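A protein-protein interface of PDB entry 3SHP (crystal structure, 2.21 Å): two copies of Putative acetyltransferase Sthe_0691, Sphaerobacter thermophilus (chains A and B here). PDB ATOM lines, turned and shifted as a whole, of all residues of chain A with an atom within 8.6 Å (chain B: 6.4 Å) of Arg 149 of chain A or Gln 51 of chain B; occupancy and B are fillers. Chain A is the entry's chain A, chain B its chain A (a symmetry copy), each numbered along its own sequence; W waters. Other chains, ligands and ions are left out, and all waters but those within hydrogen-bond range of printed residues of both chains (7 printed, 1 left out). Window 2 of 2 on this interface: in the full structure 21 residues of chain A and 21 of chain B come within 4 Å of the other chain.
The backbone NH (N) of Arg 147 of chain A lies within hydrogen-bond range of the backbone carbonyl oxygen (O) of Glu 43 of chain B (2.9 Å).
O of Arg 149 of chain A is in hydrogen-bond range of ND2 of Asn 38 of chain B, 2.8 Å away.
The side-chain carboxylate (OE2) of Glu 43 of chain B is in salt-bridge range of the guanidinium group (NE) of Arg 149 of chain A, at 2.8 Å.
NH1 of Arg 149 of chain A sits close to NE2 of Gln 51 of chain B, 3.3 Å away.
The guanidinium group (NH2) of Arg 149 of chain A is in salt-bridge range of the side-chain carboxylate (OE1) of Glu 79 of chain B (3.0 Å).
The guanidinium group of Arg 149 of chain A sits at hydrogen-bond distance from the side-chain hydroxyl of Ser 86 of chain B.
The guanidinium group (NH1) of Arg 147 of chain A lies within salt-bridge range of the side-chain carboxylate (OD2) of Asp 160 of chain A, 2.9 Å away.
The backbone carbonyl oxygen of Leu 161 of chain A is in hydrogen-bond range of the backbone NH of Met 148 of chain A (2.8 Å).
The backbone NH (N) of Glu 150 of chain A sits at hydrogen-bond distance from the side-chain carboxylate (OD1) of Asp 160 of chain A (3.0 Å).
The backbone carbonyl oxygen (O) of Ala 151 of chain A lies within hydrogen-bond range of the guanidinium group (NH2) of Arg 158 of chain A (3.1 Å).
The side-chain amide oxygen of Asn 38 of chain B sits close to the backbone carbonyl oxygen of Ala 40 of chain B.
The side-chain hydroxyl (OG1) of Thr 84 of chain B lies within hydrogen-bond range of the side-chain amide oxygen (OE1) of Gln 51 of chain B.
Among the printed residues, pairs that only touch across the chains: Met 148 of chain A with Arg 41 of chain B, Arg 147 of chain A with Ala 42 of chain B, Arg 158 of chain A with Val 37 of chain B, Val 146 of chain A with Glu 43 of chain B, Glu 150 of chain A with Val 37 of chain B, Arg 147 of chain A with Glu 48 of chain B, Arg 149 of chain A with Val 37 of chain B, Met 148 of chain A with Ala 42 of chain B, Val 146 of chain A with Ala 42 of chain B and Arg 149 of chain A with Arg 41 of chain B.
Gln 51 of chain B touches just one residue of chain A: Arg 149 (3.3 Å).
No residue of chain A comes within 4 Å of Gly 52 of chain B.
Of the printed residues of chain B, Val 146 of chain A touches Ala 42 (3.9 Å) and Glu 43 (3.4 Å).
Of the printed residues of chain A, Ala 42 of chain B touches Val 146, Arg 147 and Met 148.
The nearest residue of chain A that does not touch Gln 51 of chain B is Arg 147 of chain A (6.6 Å).
Of the 24 printed residues of chain B, 9 touch a printed residue of chain A.
Hydrophobic or aromatic side chains of chain B that line the printed part of chain A: Val 37 and Ala 42.
Among the printed residues, 16 pairs touch across the chains.
Among the printed residues, Asp or Glu carboxylates within 4 Å of a Lys or Arg side-chain nitrogen of the other chain: Arg 149 of chain A with Glu 43 of chain B (2.8 Å) and Arg 149 of chain A with Glu 79 of chain B (3.0 Å).
No position is printed for both chains.
Of the 16 pairs that touch across the chains among the printed residues, none has its exchanged pair printed and touching as well.
Water W1 lies within hydrogen-bond range of OE2 of Glu 43 of chain B, O of Ala 40 of chain B, NH2 of Arg 149 of chain A and OG of Ser 86 of chain B.
Water W6 lies within hydrogen-bond range of the side-chain carboxylate (OE1) of Glu 150 of chain A (2.5 Å) and the backbone carbonyl oxygen (O) of Val 37 of chain B (2.8 Å).
Water W5 lies within hydrogen-bond range of O of Val 37 of chain B (2.8 Å) and OE1 of Glu 150 of chain A (2.9 Å).
Water W4 lies within hydrogen-bond range of the backbone carbonyl oxygen of Arg 41 of chain B, the backbone carbonyl oxygen of Arg 149 of chain A and the side-chain amide nitrogen of Asn 38 of chain B.
Water W3 lies within hydrogen-bond range of the guanidinium group of Arg 147 of chain A and the side-chain carboxylate of Glu 43 of chain B.
Water W2 bridges OD2 of Asp 160 of chain A (3.0 Å) and OE1 of Glu 48 of chain B (3.0 Å).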
ATOM      1  N   ALA A 128     -37.967 -13.608 -20.856  1.00  0.00           N
ATOM      2  CA  ALA A 128     -37.123 -12.736 -20.068  1.00  0.00           C
ATOM      3  C   ALA A 128     -37.896 -11.648 -19.337  1.00  0.00           C
ATOM      4  O   ALA A 128     -37.370 -11.105 -18.403  1.00  0.00           O
ATOM      5  CB  ALA A 128     -35.970 -12.136 -20.915  1.00  0.00           C
ATOM      6  N   VAL A 146     -29.836 -21.046 -21.296  1.00  0.00           N
ATOM      7  CA  VAL A 146     -29.908 -20.737 -22.713  1.00  0.00           C
ATOM      8  C   VAL A 146     -30.633 -19.424 -22.881  1.00  0.00           C
ATOM      9  O   VAL A 146     -31.607 -19.152 -22.180  1.00  0.00           O
ATOM     10  CB  VAL A 146     -30.663 -21.851 -23.512  1.00  0.00           C
ATOM     11  CG1 VAL A 146     -30.801 -21.503 -25.018  1.00  0.00           C
ATOM     12  CG2 VAL A 146     -29.966 -23.197 -23.352  1.00  0.00           C
ATOM     13  N   ARG A 147     -30.137 -18.605 -23.803  1.00  0.00           N
ATOM     14  CA  ARG A 147     -30.819 -17.389 -24.211  1.00  0.00           C
ATOM     15  C   ARG A 147     -31.232 -17.531 -25.679  1.00  0.00           C
ATOM     16  O   ARG A 147     -30.400 -17.885 -26.531  1.00  0.00           O
ATOM     17  CB  ARG A 147     -29.890 -16.188 -24.078  1.00  0.00           C
ATOM     18  CG  ARG A 147     -30.574 -14.876 -24.429  1.00  0.00           C
ATOM     19  CD  ARG A 147     -29.596 -13.695 -24.438  1.00  0.00           C
ATOM     20  NE  ARG A 147     -28.854 -13.504 -23.187  1.00  0.00           N
ATOM     21  CZ  ARG A 147     -29.314 -12.830 -22.119  1.00  0.00           C
ATOM     22  NH1 ARG A 147     -30.547 -12.287 -22.116  1.00  0.00           N
ATOM     23  NH2 ARG A 147     -28.539 -12.698 -21.040  1.00  0.00           N
ATOM     24  N   MET A 148     -32.506 -17.277 -25.962  1.00  0.00           N
ATOM     25  CA  MET A 148     -33.000 -17.235 -27.323  1.00  0.00           C
ATOM     26  C   MET A 148     -33.417 -15.797 -27.598  1.00  0.00           C
ATOM     27  O   MET A 148     -34.491 -15.355 -27.159  1.00  0.00           O
ATOM     28  CB  MET A 148     -34.177 -18.199 -27.478  1.00  0.00           C
ATOM     29  CG  MET A 148     -33.798 -19.678 -27.191  1.00  0.00           C
ATOM     30  SD  MET A 148     -35.246 -20.906 -27.618  1.00  0.00           S
ATOM     31  CE  MET A 148     -35.433 -20.518 -29.540  1.00  0.00           C
ATOM     32  N   ARG A 149     -32.561 -15.053 -28.285  1.00  0.00           N
ATOM     33  CA  ARG A 149     -32.763 -13.596 -28.419  1.00  0.00           C
ATOM     34  C   ARG A 149     -33.994 -13.235 -29.225  1.00  0.00           C
ATOM     35  O   ARG A 149     -34.170 -13.685 -30.349  1.00  0.00           O
ATOM     36  CB  ARG A 149     -31.520 -12.851 -28.927  1.00  0.00           C
ATOM     37  CG  ARG A 149     -30.392 -12.830 -27.886  1.00  0.00           C
ATOM     38  CD  ARG A 149     -29.136 -12.073 -28.352  1.00  0.00           C
ATOM     39  NE  ARG A 149     -28.427 -12.764 -29.439  1.00  0.00           N
ATOM     40  CZ  ARG A 149     -28.405 -12.348 -30.705  1.00  0.00           C
ATOM     41  NH1 ARG A 149     -29.024 -11.232 -31.050  1.00  0.00           N
ATOM     42  NH2 ARG A 149     -27.749 -13.046 -31.629  1.00  0.00           N
ATOM     43  N   GLU A 150     -34.847 -12.441 -28.602  1.00  0.00           N
ATOM     44  CA  GLU A 150     -35.999 -11.865 -29.270  1.00  0.00           C
ATOM     45  C   GLU A 150     -36.892 -12.907 -29.861  1.00  0.00           C
ATOM     46  O   GLU A 150     -37.501 -12.698 -30.901  1.00  0.00           O
ATOM     47  CB  GLU A 150     -35.534 -10.889 -30.333  1.00  0.00           C
ATOM     48  CG  GLU A 150     -34.857  -9.728 -29.674  1.00  0.00           C
ATOM     49  CD  GLU A 150     -34.900  -8.568 -30.529  1.00  0.00           C
ATOM     50  OE1 GLU A 150     -34.381  -8.671 -31.656  1.00  0.00           O
ATOM     51  OE2 GLU A 150     -35.471  -7.562 -30.105  1.00  0.00           O
ATOM     52  N   ALA A 151     -36.988 -14.037 -29.177  1.00  0.00           N
ATOM     53  CA  ALA A 151     -37.771 -15.133 -29.671  1.00  0.00           C
ATOM     54  C   ALA A 151     -39.258 -14.906 -29.448  1.00  0.00           C
ATOM     55  O   ALA A 151     -40.069 -15.520 -30.144  1.00  0.00           O
ATOM     56  CB  ALA A 151     -37.317 -16.445 -29.016  1.00  0.00           C
ATOM     57  N   ILE A 152     -39.632 -14.048 -28.496  1.00  0.00           N
ATOM     58  CA  ILE A 152     -41.033 -13.914 -28.086  1.00  0.00           C
ATOM     59  C   ILE A 152     -41.608 -12.555 -28.505  1.00  0.00           C
ATOM     60  O   ILE A 152     -41.102 -11.508 -28.076  1.00  0.00           O
ATOM     61  CB  ILE A 152     -41.208 -14.087 -26.531  1.00  0.00           C
ATOM     62  CG1 ILE A 152     -40.573 -15.400 -25.986  1.00  0.00           C
ATOM     63  CG2 ILE A 152     -42.683 -14.010 -26.129  1.00  0.00           C
ATOM     64  CD1 ILE A 152     -41.000 -16.655 -26.717  1.00  0.00           C
ATOM     65  N   ARG A 158     -39.939  -7.306 -28.927  1.00  0.00           N
ATOM     66  CA  ARG A 158     -39.756  -8.732 -28.706  1.00  0.00           C
ATOM     67  C   ARG A 158     -38.860  -8.910 -27.509  1.00  0.00           C
ATOM     68  O   ARG A 158     -38.066  -8.026 -27.210  1.00  0.00           O
ATOM     69  CB  ARG A 158     -39.133  -9.391 -29.932  1.00  0.00           C
ATOM     70  CG  ARG A 158     -39.953  -9.165 -31.212  1.00  0.00           C
ATOM     71  CD  ARG A 158     -39.424  -9.984 -32.377  1.00  0.00           C
ATOM     72  NE  ARG A 158     -39.593 -11.432 -32.192  1.00  0.00           N
ATOM     73  CZ  ARG A 158     -40.678 -12.109 -32.542  1.00  0.00           C
ATOM     74  NH1 ARG A 158     -41.724 -11.466 -33.095  1.00  0.00           N
ATOM     75  NH2 ARG A 158     -40.720 -13.429 -32.334  1.00  0.00           N
ATOM     76  N   VAL A 159     -39.017 -10.024 -26.801  1.00  0.00           N
ATOM     77  CA  VAL A 159     -38.163 -10.332 -25.663  1.00  0.00           C
ATOM     78  C   VAL A 159     -37.556 -11.729 -25.804  1.00  0.00           C
ATOM     79  O   VAL A 159     -38.061 -12.567 -26.560  1.00  0.00           O
ATOM     80  CB  VAL A 159     -38.898 -10.211 -24.318  1.00  0.00           C
ATOM     81  CG1 VAL A 159     -39.567  -8.816 -24.181  1.00  0.00           C
ATOM     82  CG2 VAL A 159     -39.892 -11.332 -24.152  1.00  0.00           C
ATOM     83  N   ASP A 160     -36.472 -11.967 -25.080  1.00  0.00           N
ATOM     84  CA  ASP A 160     -35.781 -13.237 -25.172  1.00  0.00           C
ATOM     85  C   ASP A 160     -36.613 -14.322 -24.542  1.00  0.00           C
ATOM     86  O   ASP A 160     -37.312 -14.095 -23.554  1.00  0.00           O
ATOM     87  CB  ASP A 160     -34.429 -13.198 -24.447  1.00  0.00           C
ATOM     88  CG  ASP A 160     -33.503 -12.118 -24.962  1.00  0.00           C
ATOM     89  OD1 ASP A 160     -33.758 -11.506 -26.021  1.00  0.00           O
ATOM     90  OD2 ASP A 160     -32.500 -11.867 -24.277  1.00  0.00           O
ATOM     91  N   LEU A 161     -36.522 -15.517 -25.092  1.00  0.00           N
ATOM     92  CA  LEU A 161     -36.938 -16.695 -24.349  1.00  0.00           C
ATOM     93  C   LEU A 161     -35.713 -17.242 -23.624  1.00  0.00           C
ATOM     94  O   LEU A 161     -34.654 -17.436 -24.243  1.00  0.00           O
ATOM     95  CB  LEU A 161     -37.486 -17.771 -25.280  1.00  0.00           C
ATOM     96  CG  LEU A 161     -38.034 -18.996 -24.529  1.00  0.00           C
ATOM     97  CD1 LEU A 161     -39.173 -18.557 -23.581  1.00  0.00           C
ATOM     98  CD2 LEU A 161     -38.470 -20.148 -25.490  1.00  0.00           C
ATOM     99  N   LEU A 162     -35.861 -17.503 -22.331  1.00  0.00           N
ATOM    100  CA  LEU A 162     -34.787 -18.059 -21.538  1.00  0.00           C
ATOM    101  C   LEU A 162     -35.131 -19.483 -21.215  1.00  0.00           C
ATOM    102  O   LEU A 162     -36.301 -19.797 -21.041  1.00  0.00           O
ATOM    103  CB  LEU A 162     -34.609 -17.264 -20.240  1.00  0.00           C
ATOM    104  CG  LEU A 162     -34.336 -15.759 -20.395  1.00  0.00           C
ATOM    105  CD1 LEU A 162     -34.128 -15.066 -19.028  1.00  0.00           C
ATOM    106  CD2 LEU A 162     -33.134 -15.580 -21.278  1.00  0.00           C
ATOM    107  N   VAL B  37     -35.133 -12.563 -36.743  1.00  0.00           N
ATOM    108  CA  VAL B  37     -34.860 -11.823 -35.485  1.00  0.00           C
ATOM    109  C   VAL B  37     -33.371 -11.784 -35.132  1.00  0.00           C
ATOM    110  O   VAL B  37     -32.890 -10.804 -34.568  1.00  0.00           O
ATOM    111  CB  VAL B  37     -35.715 -12.283 -34.269  1.00  0.00           C
ATOM    112  CG1 VAL B  37     -37.199 -12.023 -34.549  1.00  0.00           C
ATOM    113  CG2 VAL B  37     -35.496 -13.778 -33.931  1.00  0.00           C
ATOM    114  N   ASN B  38     -32.647 -12.837 -35.493  1.00  0.00           N
ATOM    115  CA  ASN B  38     -31.211 -12.886 -35.250  1.00  0.00           C
ATOM    116  C   ASN B  38     -30.617 -13.876 -36.248  1.00  0.00           C
ATOM    117  O   ASN B  38     -31.371 -14.484 -37.027  1.00  0.00           O
ATOM    118  CB  ASN B  38     -30.942 -13.324 -33.799  1.00  0.00           C
ATOM    119  CG  ASN B  38     -31.698 -14.581 -33.437  1.00  0.00           C
ATOM    120  OD1 ASN B  38     -31.656 -15.599 -34.161  1.00  0.00           O
ATOM    121  ND2 ASN B  38     -32.423 -14.520 -32.331  1.00  0.00           N
ATOM    122  N   ALA B  39     -29.293 -14.020 -36.255  1.00  0.00           N
ATOM    123  CA  ALA B  39     -28.623 -14.994 -37.126  1.00  0.00           C
ATOM    124  C   ALA B  39     -28.283 -16.300 -36.403  1.00  0.00           C
ATOM    125  O   ALA B  39     -27.831 -17.248 -37.022  1.00  0.00           O
ATOM    126  CB  ALA B  39     -27.364 -14.389 -37.743  1.00  0.00           C
ATOM    127  N   ALA B  40     -28.461 -16.352 -35.091  1.00  0.00           N
ATOM    128  CA  ALA B  40     -28.415 -17.632 -34.368  1.00  0.00           C
ATOM    129  C   ALA B  40     -29.433 -17.601 -33.237  1.00  0.00           C
ATOM    130  O   ALA B  40     -29.279 -16.849 -32.259  1.00  0.00           O
ATOM    131  CB  ALA B  40     -27.013 -17.961 -33.849  1.00  0.00           C
ATOM    132  N   ARG B  41     -30.461 -18.435 -33.425  1.00  0.00           N
ATOM    133  CA  ARG B  41     -31.639 -18.634 -32.597  1.00  0.00           C
ATOM    134  C   ARG B  41     -31.508 -18.815 -31.074  1.00  0.00           C
ATOM    135  O   ARG B  41     -32.413 -18.442 -30.320  1.00  0.00           O
ATOM    136  CB  ARG B  41     -32.230 -19.962 -33.063  1.00  0.00           C
ATOM    137  CG  ARG B  41     -33.504 -19.875 -33.639  1.00  0.00           C
ATOM    138  CD  ARG B  41     -33.782 -21.218 -34.266  1.00  0.00           C
ATOM    139  NE  ARG B  41     -33.157 -21.245 -35.581  1.00  0.00           N
ATOM    140  CZ  ARG B  41     -33.666 -21.833 -36.665  1.00  0.00           C
ATOM    141  NH1 ARG B  41     -32.977 -21.773 -37.807  1.00  0.00           N
ATOM    142  NH2 ARG B  41     -34.858 -22.447 -36.618  1.00  0.00           N
ATOM    143  N   ALA B  42     -30.458 -19.523 -30.664  1.00  0.00           N
ATOM    144  CA  ALA B  42     -30.211 -19.807 -29.264  1.00  0.00           C
ATOM    145  C   ALA B  42     -28.729 -19.714 -29.029  1.00  0.00           C
ATOM    146  O   ALA B  42     -27.941 -19.779 -29.977  1.00  0.00           O
ATOM    147  CB  ALA B  42     -30.698 -21.187 -28.927  1.00  0.00           C
ATOM    148  N   GLU B  43     -28.339 -19.599 -27.760  1.00  0.00           N
ATOM    149  CA  GLU B  43     -26.933 -19.436 -27.408  1.00  0.00           C
ATOM    150  C   GLU B  43     -26.822 -19.719 -25.910  1.00  0.00           C
ATOM    151  O   GLU B  43     -27.807 -19.565 -25.182  1.00  0.00           O
ATOM    152  CB  GLU B  43     -26.475 -18.006 -27.741  1.00  0.00           C
ATOM    153  CG  GLU B  43     -27.299 -16.943 -27.016  1.00  0.00           C
ATOM    154  CD  GLU B  43     -27.149 -15.540 -27.568  1.00  0.00           C
ATOM    155  OE1 GLU B  43     -26.883 -14.634 -26.734  1.00  0.00           O
ATOM    156  OE2 GLU B  43     -27.351 -15.313 -28.798  1.00  0.00           O
ATOM    157  N   LYS B  47     -23.629 -12.820 -20.330  1.00  0.00           N
ATOM    158  CA  LYS B  47     -23.993 -11.427 -19.949  1.00  0.00           C
ATOM    159  C   LYS B  47     -24.571 -10.690 -21.143  1.00  0.00           C
ATOM    160  O   LYS B  47     -23.993 -10.727 -22.235  1.00  0.00           O
ATOM    161  CB  LYS B  47     -22.779 -10.643 -19.428  1.00  0.00           C
ATOM    162  CG  LYS B  47     -22.304 -11.021 -18.018  1.00  0.00           C
ATOM    163  CD  LYS B  47     -20.766 -10.909 -17.934  1.00  0.00           C
ATOM    164  CE  LYS B  47     -20.232 -11.059 -16.518  1.00  0.00           C
ATOM    165  NZ  LYS B  47     -20.522  -9.842 -15.711  1.00  0.00           N
ATOM    166  N   GLU B  48     -25.706 -10.027 -20.934  1.00  0.00           N
ATOM    167  CA  GLU B  48     -26.373  -9.268 -22.002  1.00  0.00           C
ATOM    168  C   GLU B  48     -25.468  -8.263 -22.698  1.00  0.00           C
ATOM    169  O   GLU B  48     -25.535  -8.101 -23.919  1.00  0.00           O
ATOM    170  CB  GLU B  48     -27.587  -8.526 -21.453  1.00  0.00           C
ATOM    171  CG  GLU B  48     -28.887  -8.944 -22.096  1.00  0.00           C
ATOM    172  CD  GLU B  48     -30.091  -8.406 -21.354  1.00  0.00           C
ATOM    173  OE1 GLU B  48     -31.026  -7.901 -22.021  1.00  0.00           O
ATOM    174  OE2 GLU B  48     -30.105  -8.487 -20.105  1.00  0.00           O
ATOM    175  N   LYS B  49     -24.622  -7.600 -21.909  1.00  0.00           N
ATOM    176  CA  LYS B  49     -23.752  -6.527 -22.405  1.00  0.00           C
ATOM    177  C   LYS B  49     -22.917  -6.950 -23.631  1.00  0.00           C
ATOM    178  O   LYS B  49     -22.630  -6.125 -24.504  1.00  0.00           O
ATOM    179  CB  LYS B  49     -22.881  -5.950 -21.274  1.00  0.00           C
ATOM    180  CG  LYS B  49     -21.686  -6.832 -20.840  1.00  0.00           C
ATOM    181  CD  LYS B  49     -20.953  -6.245 -19.605  1.00  0.00           C
ATOM    182  CE  LYS B  49     -19.739  -7.103 -19.203  1.00  0.00           C
ATOM    183  NZ  LYS B  49     -19.032  -6.625 -17.969  1.00  0.00           N
ATOM    184  N   LEU B  50     -22.562  -8.235 -23.708  1.00  0.00           N
ATOM    185  CA  LEU B  50     -21.801  -8.752 -24.844  1.00  0.00           C
ATOM    186  C   LEU B  50     -22.456  -8.475 -26.199  1.00  0.00           C
ATOM    187  O   LEU B  50     -21.760  -8.318 -27.194  1.00  0.00           O
ATOM    188  CB  LEU B  50     -21.548 -10.248 -24.692  1.00  0.00           C
ATOM    189  CG  LEU B  50     -20.715 -10.705 -23.495  1.00  0.00           C
ATOM    190  CD1 LEU B  50     -20.712 -12.224 -23.461  1.00  0.00           C
ATOM    191  CD2 LEU B  50     -19.278 -10.150 -23.548  1.00  0.00           C
ATOM    192  N   GLN B  51     -23.786  -8.403 -26.221  1.00  0.00           N
ATOM    193  CA  GLN B  51     -24.526  -8.150 -27.454  1.00  0.00           C
ATOM    194  C   GLN B  51     -24.560  -6.652 -27.802  1.00  0.00           C
ATOM    195  O   GLN B  51     -24.657  -6.286 -28.977  1.00  0.00           O
ATOM    196  CB  GLN B  51     -25.952  -8.692 -27.343  1.00  0.00           C
ATOM    197  CG  GLN B  51     -26.669  -8.896 -28.691  1.00  0.00           C
ATOM    198  CD  GLN B  51     -26.052 -10.018 -29.508  1.00  0.00           C
ATOM    199  OE1 GLN B  51     -25.605 -11.029 -28.964  1.00  0.00           O
ATOM    200  NE2 GLN B  51     -26.006  -9.833 -30.819  1.00  0.00           N
ATOM    201  N   GLY B  52     -24.481  -5.799 -26.782  1.00  0.00           N
ATOM    202  CA  GLY B  52     -24.592  -4.357 -26.966  1.00  0.00           C
ATOM    203  C   GLY B  52     -25.990  -3.890 -27.347  1.00  0.00           C
ATOM    204  O   GLY B  52     -26.952  -4.658 -27.285  1.00  0.00           O
ATOM    205  N   ASP B  53     -26.089  -2.629 -27.767  1.00  0.00           N
ATOM    206  CA  ASP B  53     -27.362  -2.007 -28.169  1.00  0.00           C
ATOM    207  C   ASP B  53     -27.821  -2.396 -29.595  1.00  0.00           C
ATOM    208  O   ASP B  53     -26.990  -2.569 -30.497  1.00  0.00           O
ATOM    209  CB  ASP B  53     -27.252  -0.483 -28.027  1.00  0.00           C
ATOM    210  CG  ASP B  53     -27.036  -0.048 -26.571  1.00  0.00           C
ATOM    211  OD1 ASP B  53     -27.423  -0.813 -25.644  1.00  0.00           O
ATOM    212  OD2 ASP B  53     -26.479   1.052 -26.347  1.00  0.00           O
ATOM    213  N   PRO B  54     -29.146  -2.556 -29.792  1.00  0.00           N
ATOM    214  CA  PRO B  54     -29.692  -2.893 -31.121  1.00  0.00           C
ATOM    215  C   PRO B  54     -29.387  -1.859 -32.230  1.00  0.00           C
ATOM    216  O   PRO B  54     -29.189  -2.236 -33.383  1.00  0.00           O
ATOM    217  CB  PRO B  54     -31.205  -3.024 -30.873  1.00  0.00           C
ATOM    218  CG  PRO B  54     -31.442  -2.589 -29.427  1.00  0.00           C
ATOM    219  CD  PRO B  54     -30.141  -2.746 -28.718  1.00  0.00           C
ATOM    220  N   ASP B  56     -26.690  -0.443 -32.553  1.00  0.00           N
ATOM    221  CA  ASP B  56     -25.295  -0.713 -32.927  1.00  0.00           C
ATOM    222  C   ASP B  56     -25.043  -2.079 -33.577  1.00  0.00           C
ATOM    223  O   ASP B  56     -23.916  -2.380 -33.985  1.00  0.00           O
ATOM    224  CB  ASP B  56     -24.396  -0.556 -31.708  1.00  0.00           C
ATOM    225  CG  ASP B  56     -24.505   0.819 -31.091  1.00  0.00           C
ATOM    226  OD1 ASP B  56     -24.591   1.801 -31.859  1.00  0.00           O
ATOM    227  OD2 ASP B  56     -24.514   0.915 -29.842  1.00  0.00           O
ATOM    228  N   ALA B  57     -26.079  -2.903 -33.663  1.00  0.00           N
ATOM    229  CA  ALA B  57     -25.966  -4.201 -34.314  1.00  0.00           C
ATOM    230  C   ALA B  57     -25.633  -4.021 -35.807  1.00  0.00           C
ATOM    231  O   ALA B  57     -26.096  -3.062 -36.452  1.00  0.00           O
ATOM    232  CB  ALA B  57     -27.246  -4.980 -34.134  1.00  0.00           C
ATOM    233  N   GLU B  79     -24.634 -11.786 -37.970  1.00  0.00           N
ATOM    234  CA  GLU B  79     -25.115 -10.675 -37.143  1.00  0.00           C
ATOM    235  C   GLU B  79     -24.079 -10.355 -36.060  1.00  0.00           C
ATOM    236  O   GLU B  79     -23.767 -11.208 -35.226  1.00  0.00           O
ATOM    237  CB  GLU B  79     -26.501 -11.018 -36.546  1.00  0.00           C
ATOM    238  CG  GLU B  79     -26.989 -10.062 -35.472  1.00  0.00           C
ATOM    239  CD  GLU B  79     -27.933 -10.699 -34.442  1.00  0.00           C
ATOM    240  OE1 GLU B  79     -28.044 -11.955 -34.365  1.00  0.00           O
ATOM    241  OE2 GLU B  79     -28.559  -9.918 -33.691  1.00  0.00           O
ATOM    242  N   PHE B  80     -23.509  -9.158 -36.103  1.00  0.00           N
ATOM    243  CA  PHE B  80     -22.572  -8.745 -35.061  1.00  0.00           C
ATOM    244  C   PHE B  80     -23.311  -8.011 -33.962  1.00  0.00           C
ATOM    245  O   PHE B  80     -24.222  -7.212 -34.234  1.00  0.00           O
ATOM    246  CB  PHE B  80     -21.449  -7.825 -35.581  1.00  0.00           C
ATOM    247  CG  PHE B  80     -20.476  -8.505 -36.502  1.00  0.00           C
ATOM    248  CD1 PHE B  80     -20.447  -8.183 -37.856  1.00  0.00           C
ATOM    249  CD2 PHE B  80     -19.594  -9.468 -36.024  1.00  0.00           C
ATOM    250  CE1 PHE B  80     -19.566  -8.808 -38.723  1.00  0.00           C
ATOM    251  CE2 PHE B  80     -18.694 -10.113 -36.896  1.00  0.00           C
ATOM    252  CZ  PHE B  80     -18.686  -9.780 -38.247  1.00  0.00           C
ATOM    253  N   GLY B  81     -22.926  -8.290 -32.726  1.00  0.00           N
ATOM    254  CA  GLY B  81     -23.244  -7.406 -31.620  1.00  0.00           C
ATOM    255  C   GLY B  81     -21.962  -6.671 -31.230  1.00  0.00           C
ATOM    256  O   GLY B  81     -21.045  -6.531 -32.034  1.00  0.00           O
ATOM    257  N   LYS B  82     -21.862  -6.222 -29.989  1.00  0.00           N
ATOM    258  CA  LYS B  82     -20.655  -5.520 -29.576  1.00  0.00           C
ATOM    259  C   LYS B  82     -19.427  -6.427 -29.599  1.00  0.00           C
ATOM    260  O   LYS B  82     -18.415  -6.081 -30.200  1.00  0.00           O
ATOM    261  CB  LYS B  82     -20.838  -4.882 -28.202  1.00  0.00           C
ATOM    262  CG  LYS B  82     -19.684  -4.002 -27.765  1.00  0.00           C
ATOM    263  CD  LYS B  82     -20.055  -3.211 -26.515  1.00  0.00           C
ATOM    264  CE  LYS B  82     -20.440  -4.122 -25.320  1.00  0.00           C
ATOM    265  NZ  LYS B  82     -21.188  -3.409 -24.198  1.00  0.00           N
ATOM    266  N   GLN B  83     -19.519  -7.580 -28.953  1.00  0.00           N
ATOM    267  CA  GLN B  83     -18.403  -8.498 -28.897  1.00  0.00           C
ATOM    268  C   GLN B  83     -18.767  -9.897 -29.384  1.00  0.00           C
ATOM    269  O   GLN B  83     -18.088 -10.869 -29.039  1.00  0.00           O
ATOM    270  CB  GLN B  83     -17.906  -8.543 -27.462  1.00  0.00           C
ATOM    271  CG  GLN B  83     -16.897  -7.422 -27.186  1.00  0.00           C
ATOM    272  CD  GLN B  83     -16.932  -6.922 -25.773  1.00  0.00           C
ATOM    273  OE1 GLN B  83     -17.894  -7.149 -25.026  1.00  0.00           O
ATOM    274  NE2 GLN B  83     -15.889  -6.204 -25.393  1.00  0.00           N
ATOM    275  N   THR B  84     -19.851  -9.990 -30.163  1.00  0.00           N
ATOM    276  CA  THR B  84     -20.395 -11.281 -30.586  1.00  0.00           C
ATOM    277  C   THR B  84     -20.557 -11.354 -32.087  1.00  0.00           C
ATOM    278  O   THR B  84     -20.753 -10.331 -32.746  1.00  0.00           O
ATOM    279  CB  THR B  84     -21.774 -11.558 -29.954  1.00  0.00           C
ATOM    280  OG1 THR B  84     -22.713 -10.578 -30.410  1.00  0.00           O
ATOM    281  CG2 THR B  84     -21.698 -11.508 -28.414  1.00  0.00           C
ATOM    282  N   SER B  86     -22.846 -13.962 -34.680  1.00  0.00           N
ATOM    283  CA  SER B  86     -23.784 -15.058 -34.819  1.00  0.00           C
ATOM    284  C   SER B  86     -24.033 -15.277 -36.305  1.00  0.00           C
ATOM    285  O   SER B  86     -24.118 -14.318 -37.070  1.00  0.00           O
ATOM    286  CB  SER B  86     -25.092 -14.721 -34.100  1.00  0.00           C
ATOM    287  OG  SER B  86     -24.838 -14.415 -32.738  1.00  0.00           O
HETATM  288  O   HOH W   1     -26.939 -15.733 -31.203  1.00  0.00           O
HETATM  289  O   HOH W   2     -33.251  -9.894 -22.170  1.00  0.00           O
HETATM  290  O   HOH W   3     -26.418 -14.760 -23.778  1.00  0.00           O
HETATM  291  O   HOH W   4     -34.391 -16.564 -30.934  1.00  0.00           O
HETATM  292  O   HOH W   5     -32.416 -10.779 -31.838  1.00  0.00           O
HETATM  293  O   HOH W   6     -34.036  -8.333 -34.133  1.00  0.00           O
HETATM  294  O   HOH W   7     -30.262 -11.024 -19.170  1.00  0.00           O
